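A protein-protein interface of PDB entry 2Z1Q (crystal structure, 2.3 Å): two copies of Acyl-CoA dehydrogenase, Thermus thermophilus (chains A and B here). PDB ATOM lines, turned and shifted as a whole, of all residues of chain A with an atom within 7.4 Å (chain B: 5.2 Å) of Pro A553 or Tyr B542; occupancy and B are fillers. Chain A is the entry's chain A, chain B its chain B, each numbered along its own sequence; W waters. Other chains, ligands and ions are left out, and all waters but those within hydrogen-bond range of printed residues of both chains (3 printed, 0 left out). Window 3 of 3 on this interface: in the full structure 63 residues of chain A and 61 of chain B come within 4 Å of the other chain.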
ATOM      1  N   GLN A 449     -36.571   2.767  -3.422  1.00  0.00           N
ATOM      2  CA  GLN A 449     -37.133   4.043  -3.836  1.00  0.00           C
ATOM      3  C   GLN A 449     -38.621   3.915  -4.122  1.00  0.00           C
ATOM      4  O   GLN A 449     -39.380   4.861  -3.917  1.00  0.00           O
ATOM      5  CB  GLN A 449     -36.405   4.553  -5.074  1.00  0.00           C
ATOM      6  CG  GLN A 449     -35.032   5.098  -4.774  1.00  0.00           C
ATOM      7  CD  GLN A 449     -34.150   5.125  -5.999  1.00  0.00           C
ATOM      8  OE1 GLN A 449     -33.055   5.692  -5.976  1.00  0.00           O
ATOM      9  NE2 GLN A 449     -34.613   4.496  -7.076  1.00  0.00           N
ATOM     10  N   ALA A 515     -36.884   6.852 -12.654  1.00  0.00           N
ATOM     11  CA  ALA A 515     -36.115   8.089 -12.493  1.00  0.00           C
ATOM     12  C   ALA A 515     -37.001   9.316 -12.539  1.00  0.00           C
ATOM     13  O   ALA A 515     -36.904  10.197 -11.682  1.00  0.00           O
ATOM     14  CB  ALA A 515     -35.031   8.210 -13.563  1.00  0.00           C
ATOM     15  N   ARG A 551     -32.229  10.076  -4.273  1.00  0.00           N
ATOM     16  CA  ARG A 551     -31.699   9.070  -5.182  1.00  0.00           C
ATOM     17  C   ARG A 551     -30.568   9.610  -6.040  1.00  0.00           C
ATOM     18  O   ARG A 551     -30.404  10.821  -6.187  1.00  0.00           O
ATOM     19  CB  ARG A 551     -32.793   8.551  -6.110  1.00  0.00           C
ATOM     20  CG  ARG A 551     -33.129   9.491  -7.273  1.00  0.00           C
ATOM     21  CD  ARG A 551     -33.785  10.763  -6.774  1.00  0.00           C
ATOM     22  NE  ARG A 551     -34.208  11.654  -7.849  1.00  0.00           N
ATOM     23  CZ  ARG A 551     -34.898  12.777  -7.656  1.00  0.00           C
ATOM     24  NH1 ARG A 551     -35.246  13.540  -8.682  1.00  0.00           N
ATOM     25  NH2 ARG A 551     -35.245  13.142  -6.422  1.00  0.00           N
ATOM     26  N   GLU A 552     -29.799   8.696  -6.618  1.00  0.00           N
ATOM     27  CA  GLU A 552     -28.704   9.081  -7.495  1.00  0.00           C
ATOM     28  C   GLU A 552     -29.218   9.249  -8.916  1.00  0.00           C
ATOM     29  O   GLU A 552     -30.022   8.455  -9.402  1.00  0.00           O
ATOM     30  CB  GLU A 552     -27.593   8.031  -7.485  1.00  0.00           C
ATOM     31  CG  GLU A 552     -26.719   8.066  -6.242  1.00  0.00           C
ATOM     32  CD  GLU A 552     -26.063   9.418  -6.027  1.00  0.00           C
ATOM     33  OE1 GLU A 552     -25.203   9.803  -6.850  1.00  0.00           O
ATOM     34  OE2 GLU A 552     -26.408  10.095  -5.034  1.00  0.00           O
ATOM     35  N   PRO A 553     -28.749  10.293  -9.602  1.00  0.00           N
ATOM     36  CA  PRO A 553     -29.160  10.570 -10.977  1.00  0.00           C
ATOM     37  C   PRO A 553     -28.703   9.511 -11.977  1.00  0.00           C
ATOM     38  O   PRO A 553     -27.544   9.086 -11.969  1.00  0.00           O
ATOM     39  CB  PRO A 553     -28.549  11.942 -11.245  1.00  0.00           C
ATOM     40  CG  PRO A 553     -27.310  11.915 -10.405  1.00  0.00           C
ATOM     41  CD  PRO A 553     -27.807  11.316  -9.117  1.00  0.00           C
ATOM     42  N   GLY A 554     -29.631   9.089 -12.830  1.00  0.00           N
ATOM     43  CA  GLY A 554     -29.335   8.088 -13.839  1.00  0.00           C
ATOM     44  C   GLY A 554     -29.019   8.730 -15.181  1.00  0.00           C
ATOM     45  O   GLY A 554     -29.381   9.887 -15.421  1.00  0.00           O
ATOM     46  N   ASP A 555     -28.354   7.987 -16.065  1.00  0.00           N
ATOM     47  CA  ASP A 555     -27.996   8.516 -17.375  1.00  0.00           C
ATOM     48  C   ASP A 555     -29.160   8.343 -18.353  1.00  0.00           C
ATOM     49  O   ASP A 555     -29.135   7.470 -19.222  1.00  0.00           O
ATOM     50  CB  ASP A 555     -26.749   7.814 -17.927  1.00  0.00           C
ATOM     51  CG  ASP A 555     -26.121   8.577 -19.089  1.00  0.00           C
ATOM     52  OD1 ASP A 555     -26.835   9.395 -19.712  1.00  0.00           O
ATOM     53  OD2 ASP A 555     -24.923   8.366 -19.388  1.00  0.00           O
ATOM     54  N   LEU A 556     -30.177   9.188 -18.200  1.00  0.00           N
ATOM     55  CA  LEU A 556     -31.356   9.126 -19.055  1.00  0.00           C
ATOM     56  C   LEU A 556     -30.985   9.248 -20.530  1.00  0.00           C
ATOM     57  O   LEU A 556     -31.686   8.742 -21.391  1.00  0.00           O
ATOM     58  CB  LEU A 556     -32.368  10.205 -18.648  1.00  0.00           C
ATOM     59  CG  LEU A 556     -33.066   9.990 -17.292  1.00  0.00           C
ATOM     60  CD1 LEU A 556     -33.974  11.171 -17.011  1.00  0.00           C
ATOM     61  CD2 LEU A 556     -33.872   8.688 -17.288  1.00  0.00           C
ATOM     62  N   LEU B 526     -30.048  17.400 -14.221  1.00  0.00           N
ATOM     63  CA  LEU B 526     -29.664  16.113 -13.667  1.00  0.00           C
ATOM     64  C   LEU B 526     -29.940  14.927 -14.579  1.00  0.00           C
ATOM     65  O   LEU B 526     -29.426  13.832 -14.341  1.00  0.00           O
ATOM     66  CB  LEU B 526     -30.356  15.891 -12.321  1.00  0.00           C
ATOM     67  CG  LEU B 526     -29.958  16.886 -11.231  1.00  0.00           C
ATOM     68  CD1 LEU B 526     -30.873  16.719 -10.022  1.00  0.00           C
ATOM     69  CD2 LEU B 526     -28.497  16.669 -10.861  1.00  0.00           C
ATOM     70  N   LEU B 529     -26.623  15.288 -16.989  1.00  0.00           N
ATOM     71  CA  LEU B 529     -25.312  15.464 -16.381  1.00  0.00           C
ATOM     72  C   LEU B 529     -24.493  14.168 -16.302  1.00  0.00           C
ATOM     73  O   LEU B 529     -23.293  14.167 -16.587  1.00  0.00           O
ATOM     74  CB  LEU B 529     -25.474  16.103 -15.001  1.00  0.00           C
ATOM     75  CG  LEU B 529     -24.871  17.502 -14.815  1.00  0.00           C
ATOM     76  CD1 LEU B 529     -24.608  18.203 -16.146  1.00  0.00           C
ATOM     77  CD2 LEU B 529     -25.824  18.308 -13.968  1.00  0.00           C
ATOM     78  N   PRO B 530     -25.130  13.053 -15.918  1.00  0.00           N
ATOM     79  CA  PRO B 530     -24.421  11.771 -15.826  1.00  0.00           C
ATOM     80  C   PRO B 530     -23.755  11.441 -17.166  1.00  0.00           C
ATOM     81  O   PRO B 530     -22.869  10.577 -17.239  1.00  0.00           O
ATOM     82  CB  PRO B 530     -25.538  10.785 -15.480  1.00  0.00           C
ATOM     83  CG  PRO B 530     -26.510  11.629 -14.701  1.00  0.00           C
ATOM     84  CD  PRO B 530     -26.534  12.917 -15.485  1.00  0.00           C
ATOM     85  N   VAL B 533     -20.363  13.881 -16.769  1.00  0.00           N
ATOM     86  CA  VAL B 533     -19.454  13.622 -15.649  1.00  0.00           C
ATOM     87  C   VAL B 533     -19.691  12.274 -14.975  1.00  0.00           C
ATOM     88  O   VAL B 533     -20.793  11.727 -15.031  1.00  0.00           O
ATOM     89  CB  VAL B 533     -19.571  14.728 -14.566  1.00  0.00           C
ATOM     90  CG1 VAL B 533     -18.930  16.015 -15.061  1.00  0.00           C
ATOM     91  CG2 VAL B 533     -21.034  14.973 -14.221  1.00  0.00           C
ATOM     92  N   ALA B 538     -18.449  13.775 -10.706  1.00  0.00           N
ATOM     93  CA  ALA B 538     -19.867  13.897 -11.050  1.00  0.00           C
ATOM     94  C   ALA B 538     -20.724  14.327  -9.859  1.00  0.00           C
ATOM     95  O   ALA B 538     -21.597  15.183  -9.988  1.00  0.00           O
ATOM     96  CB  ALA B 538     -20.389  12.580 -11.609  1.00  0.00           C
ATOM     97  N   ARG B 539     -20.468  13.728  -8.703  1.00  0.00           N
ATOM     98  CA  ARG B 539     -21.225  14.053  -7.500  1.00  0.00           C
ATOM     99  C   ARG B 539     -21.132  15.533  -7.148  1.00  0.00           C
ATOM    100  O   ARG B 539     -22.124  16.142  -6.752  1.00  0.00           O
ATOM    101  CB  ARG B 539     -20.727  13.215  -6.325  1.00  0.00           C
ATOM    102  CG  ARG B 539     -20.900  11.726  -6.540  1.00  0.00           C
ATOM    103  CD  ARG B 539     -21.801  11.143  -5.477  1.00  0.00           C
ATOM    104  NE  ARG B 539     -21.150  11.121  -4.171  1.00  0.00           N
ATOM    105  CZ  ARG B 539     -21.791  10.936  -3.020  1.00  0.00           C
ATOM    106  NH1 ARG B 539     -23.109  10.758  -3.011  1.00  0.00           N
ATOM    107  NH2 ARG B 539     -21.111  10.916  -1.879  1.00  0.00           N
ATOM    108  N   VAL B 540     -19.939  16.107  -7.302  1.00  0.00           N
ATOM    109  CA  VAL B 540     -19.718  17.525  -7.004  1.00  0.00           C
ATOM    110  C   VAL B 540     -20.603  18.365  -7.920  1.00  0.00           C
ATOM    111  O   VAL B 540     -21.285  19.292  -7.473  1.00  0.00           O
ATOM    112  CB  VAL B 540     -18.240  17.950  -7.246  1.00  0.00           C
ATOM    113  CG1 VAL B 540     -18.009  19.349  -6.687  1.00  0.00           C
ATOM    114  CG2 VAL B 540     -17.281  16.958  -6.600  1.00  0.00           C
ATOM    115  N   VAL B 541     -20.583  18.033  -9.206  1.00  0.00           N
ATOM    116  CA  VAL B 541     -21.394  18.730 -10.201  1.00  0.00           C
ATOM    117  C   VAL B 541     -22.877  18.616  -9.852  1.00  0.00           C
ATOM    118  O   VAL B 541     -23.619  19.596  -9.954  1.00  0.00           O
ATOM    119  CB  VAL B 541     -21.166  18.138 -11.613  1.00  0.00           C
ATOM    120  CG1 VAL B 541     -22.046  18.851 -12.638  1.00  0.00           C
ATOM    121  CG2 VAL B 541     -19.688  18.250 -11.989  1.00  0.00           C
ATOM    122  N   TYR B 542     -23.313  17.428  -9.434  1.00  0.00           N
ATOM    123  CA  TYR B 542     -24.718  17.236  -9.088  1.00  0.00           C
ATOM    124  C   TYR B 542     -25.143  18.152  -7.940  1.00  0.00           C
ATOM    125  O   TYR B 542     -26.244  18.714  -7.960  1.00  0.00           O
ATOM    126  CB  TYR B 542     -25.004  15.768  -8.714  1.00  0.00           C
ATOM    127  CG  TYR B 542     -24.676  14.748  -9.792  1.00  0.00           C
ATOM    128  CD1 TYR B 542     -24.650  15.094 -11.149  1.00  0.00           C
ATOM    129  CD2 TYR B 542     -24.418  13.420  -9.451  1.00  0.00           C
ATOM    130  CE1 TYR B 542     -24.375  14.130 -12.140  1.00  0.00           C
ATOM    131  CE2 TYR B 542     -24.144  12.457 -10.424  1.00  0.00           C
ATOM    132  CZ  TYR B 542     -24.125  12.813 -11.760  1.00  0.00           C
ATOM    133  OH  TYR B 542     -23.852  11.836 -12.690  1.00  0.00           O
ATOM    134  N   SER B 543     -24.283  18.313  -6.942  1.00  0.00           N
ATOM    135  CA  SER B 543     -24.613  19.181  -5.824  1.00  0.00           C
ATOM    136  C   SER B 543     -24.668  20.632  -6.302  1.00  0.00           C
ATOM    137  O   SER B 543     -25.482  21.418  -5.824  1.00  0.00           O
ATOM    138  CB  SER B 543     -23.578  19.040  -4.706  1.00  0.00           C
ATOM    139  OG  SER B 543     -23.618  17.736  -4.152  1.00  0.00           O
ATOM    140  N   ALA B 544     -23.817  20.993  -7.255  1.00  0.00           N
ATOM    141  CA  ALA B 544     -23.836  22.366  -7.741  1.00  0.00           C
ATOM    142  C   ALA B 544     -25.119  22.639  -8.517  1.00  0.00           C
ATOM    143  O   ALA B 544     -25.694  23.723  -8.412  1.00  0.00           O
ATOM    144  CB  ALA B 544     -22.634  22.636  -8.614  1.00  0.00           C
ATOM    145  N   ALA B 545     -25.564  21.652  -9.290  1.00  0.00           N
ATOM    146  CA  ALA B 545     -26.783  21.801 -10.069  1.00  0.00           C
ATOM    147  C   ALA B 545     -27.978  21.982  -9.135  1.00  0.00           C
ATOM    148  O   ALA B 545     -28.906  22.735  -9.436  1.00  0.00           O
ATOM    149  CB  ALA B 545     -26.984  20.575 -10.967  1.00  0.00           C
ATOM    150  N   ARG B 546     -27.951  21.307  -7.991  1.00  0.00           N
ATOM    151  CA  ARG B 546     -29.052  21.407  -7.038  1.00  0.00           C
ATOM    152  C   ARG B 546     -29.104  22.751  -6.335  1.00  0.00           C
ATOM    153  O   ARG B 546     -30.178  23.328  -6.164  1.00  0.00           O
ATOM    154  CB  ARG B 546     -28.966  20.301  -5.985  1.00  0.00           C
ATOM    155  CG  ARG B 546     -29.044  18.896  -6.557  1.00  0.00           C
ATOM    156  CD  ARG B 546     -29.282  17.861  -5.462  1.00  0.00           C
ATOM    157  NE  ARG B 546     -29.266  16.498  -5.991  1.00  0.00           N
ATOM    158  CZ  ARG B 546     -28.161  15.832  -6.313  1.00  0.00           C
ATOM    159  NH1 ARG B 546     -28.248  14.597  -6.793  1.00  0.00           N
ATOM    160  NH2 ARG B 546     -26.968  16.393  -6.136  1.00  0.00           N
HETATM  161  O   HOH W   1     -30.816  13.347  -7.952  1.00  0.00           O
HETATM  162  O   HOH W   2     -30.951  11.722 -13.572  1.00  0.00           O
HETATM  163  O   HOH W   3     -26.041  12.577  -5.851  1.00  0.00           O
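Of the 13 printed residues of chain B, 4 touch a printed residue of chain A.
Hydrophobic or aromatic side chains of chain B that line the printed part of chain A: Pro B530 and Tyr B542.
Of the 8 printed residues of chain A, 4 touch a printed residue of chain B.
Among the printed residues, 6 pairs touch across the chains.
Among the printed residues, Asp or Glu carboxylates within 4 Å of a Lys or Arg side-chain nitrogen of the other chain: Glu A552 with Arg B539.
No position is printed for both chains.
Of the 6 pairs that touch across the chains among the printed residues, none has its exchanged pair printed and touching as well.
O of Arg B539 sits at hydrogen-bond distance from OG of Ser B543, at 3.4 Å.
The guanidinium group (NH2) of Arg B546 lies within hydrogen-bond range of the backbone carbonyl oxygen (O) of Tyr B542 (3.0 Å).
Of the printed residues of chain B, Glu A552 touches Arg B539.
Of chain B, only Leu B526, Pro B530 and Tyr B542 come within 4 Å of Pro A553.
Of the printed residues of chain B, Asp A555 touches Pro B530.
Printed residues of chain A within 4 Å of Leu B526: Pro A553 (3.7 Å).
Of the printed residues of chain A, Pro B530 touches Pro A553, Gly A554 and Asp A555.
Of the printed residues of chain A, Arg B539 touches Glu A552.
Tyr B542 touches just one residue of chain A: Pro A553.
Arg B546 touches none of the printed residues of chain A.
The nearest residue of chain B that does not touch Pro A553 is Arg B546 (4.04 Å).
The nearest printed residue of chain A that does not touch Arg B539 is Pro A553 (7.0 Å).
Water W3 bridges the side-chain carboxylate (OE2) of Glu A552 and the guanidinium group (NH1) of Arg B546.
Water W2 lies within hydrogen-bond range of the backbone carbonyl oxygen (O) of Leu B526 and the backbone NH (N) of Gly A554.
Water W1 bridges the guanidinium group (NH1) of Arg B546 (3.1 Å) and the backbone carbonyl oxygen (O) of Arg A551 (3.1 Å).
NH1 of Arg B539 is in salt-bridge range of OE2 of Glu A552, 3.9 Å away.
Among the printed residues, merely in contact across the chains: Pro A553 with Leu B526 (3.7 Å), Pro A553 with Pro B530 (3.9 Å), Pro A553 with Tyr B542 (3.2 Å), Gly A554 with Pro B530 (3.4 Å) and Asp A555 with Pro B530 (3.7 Å).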
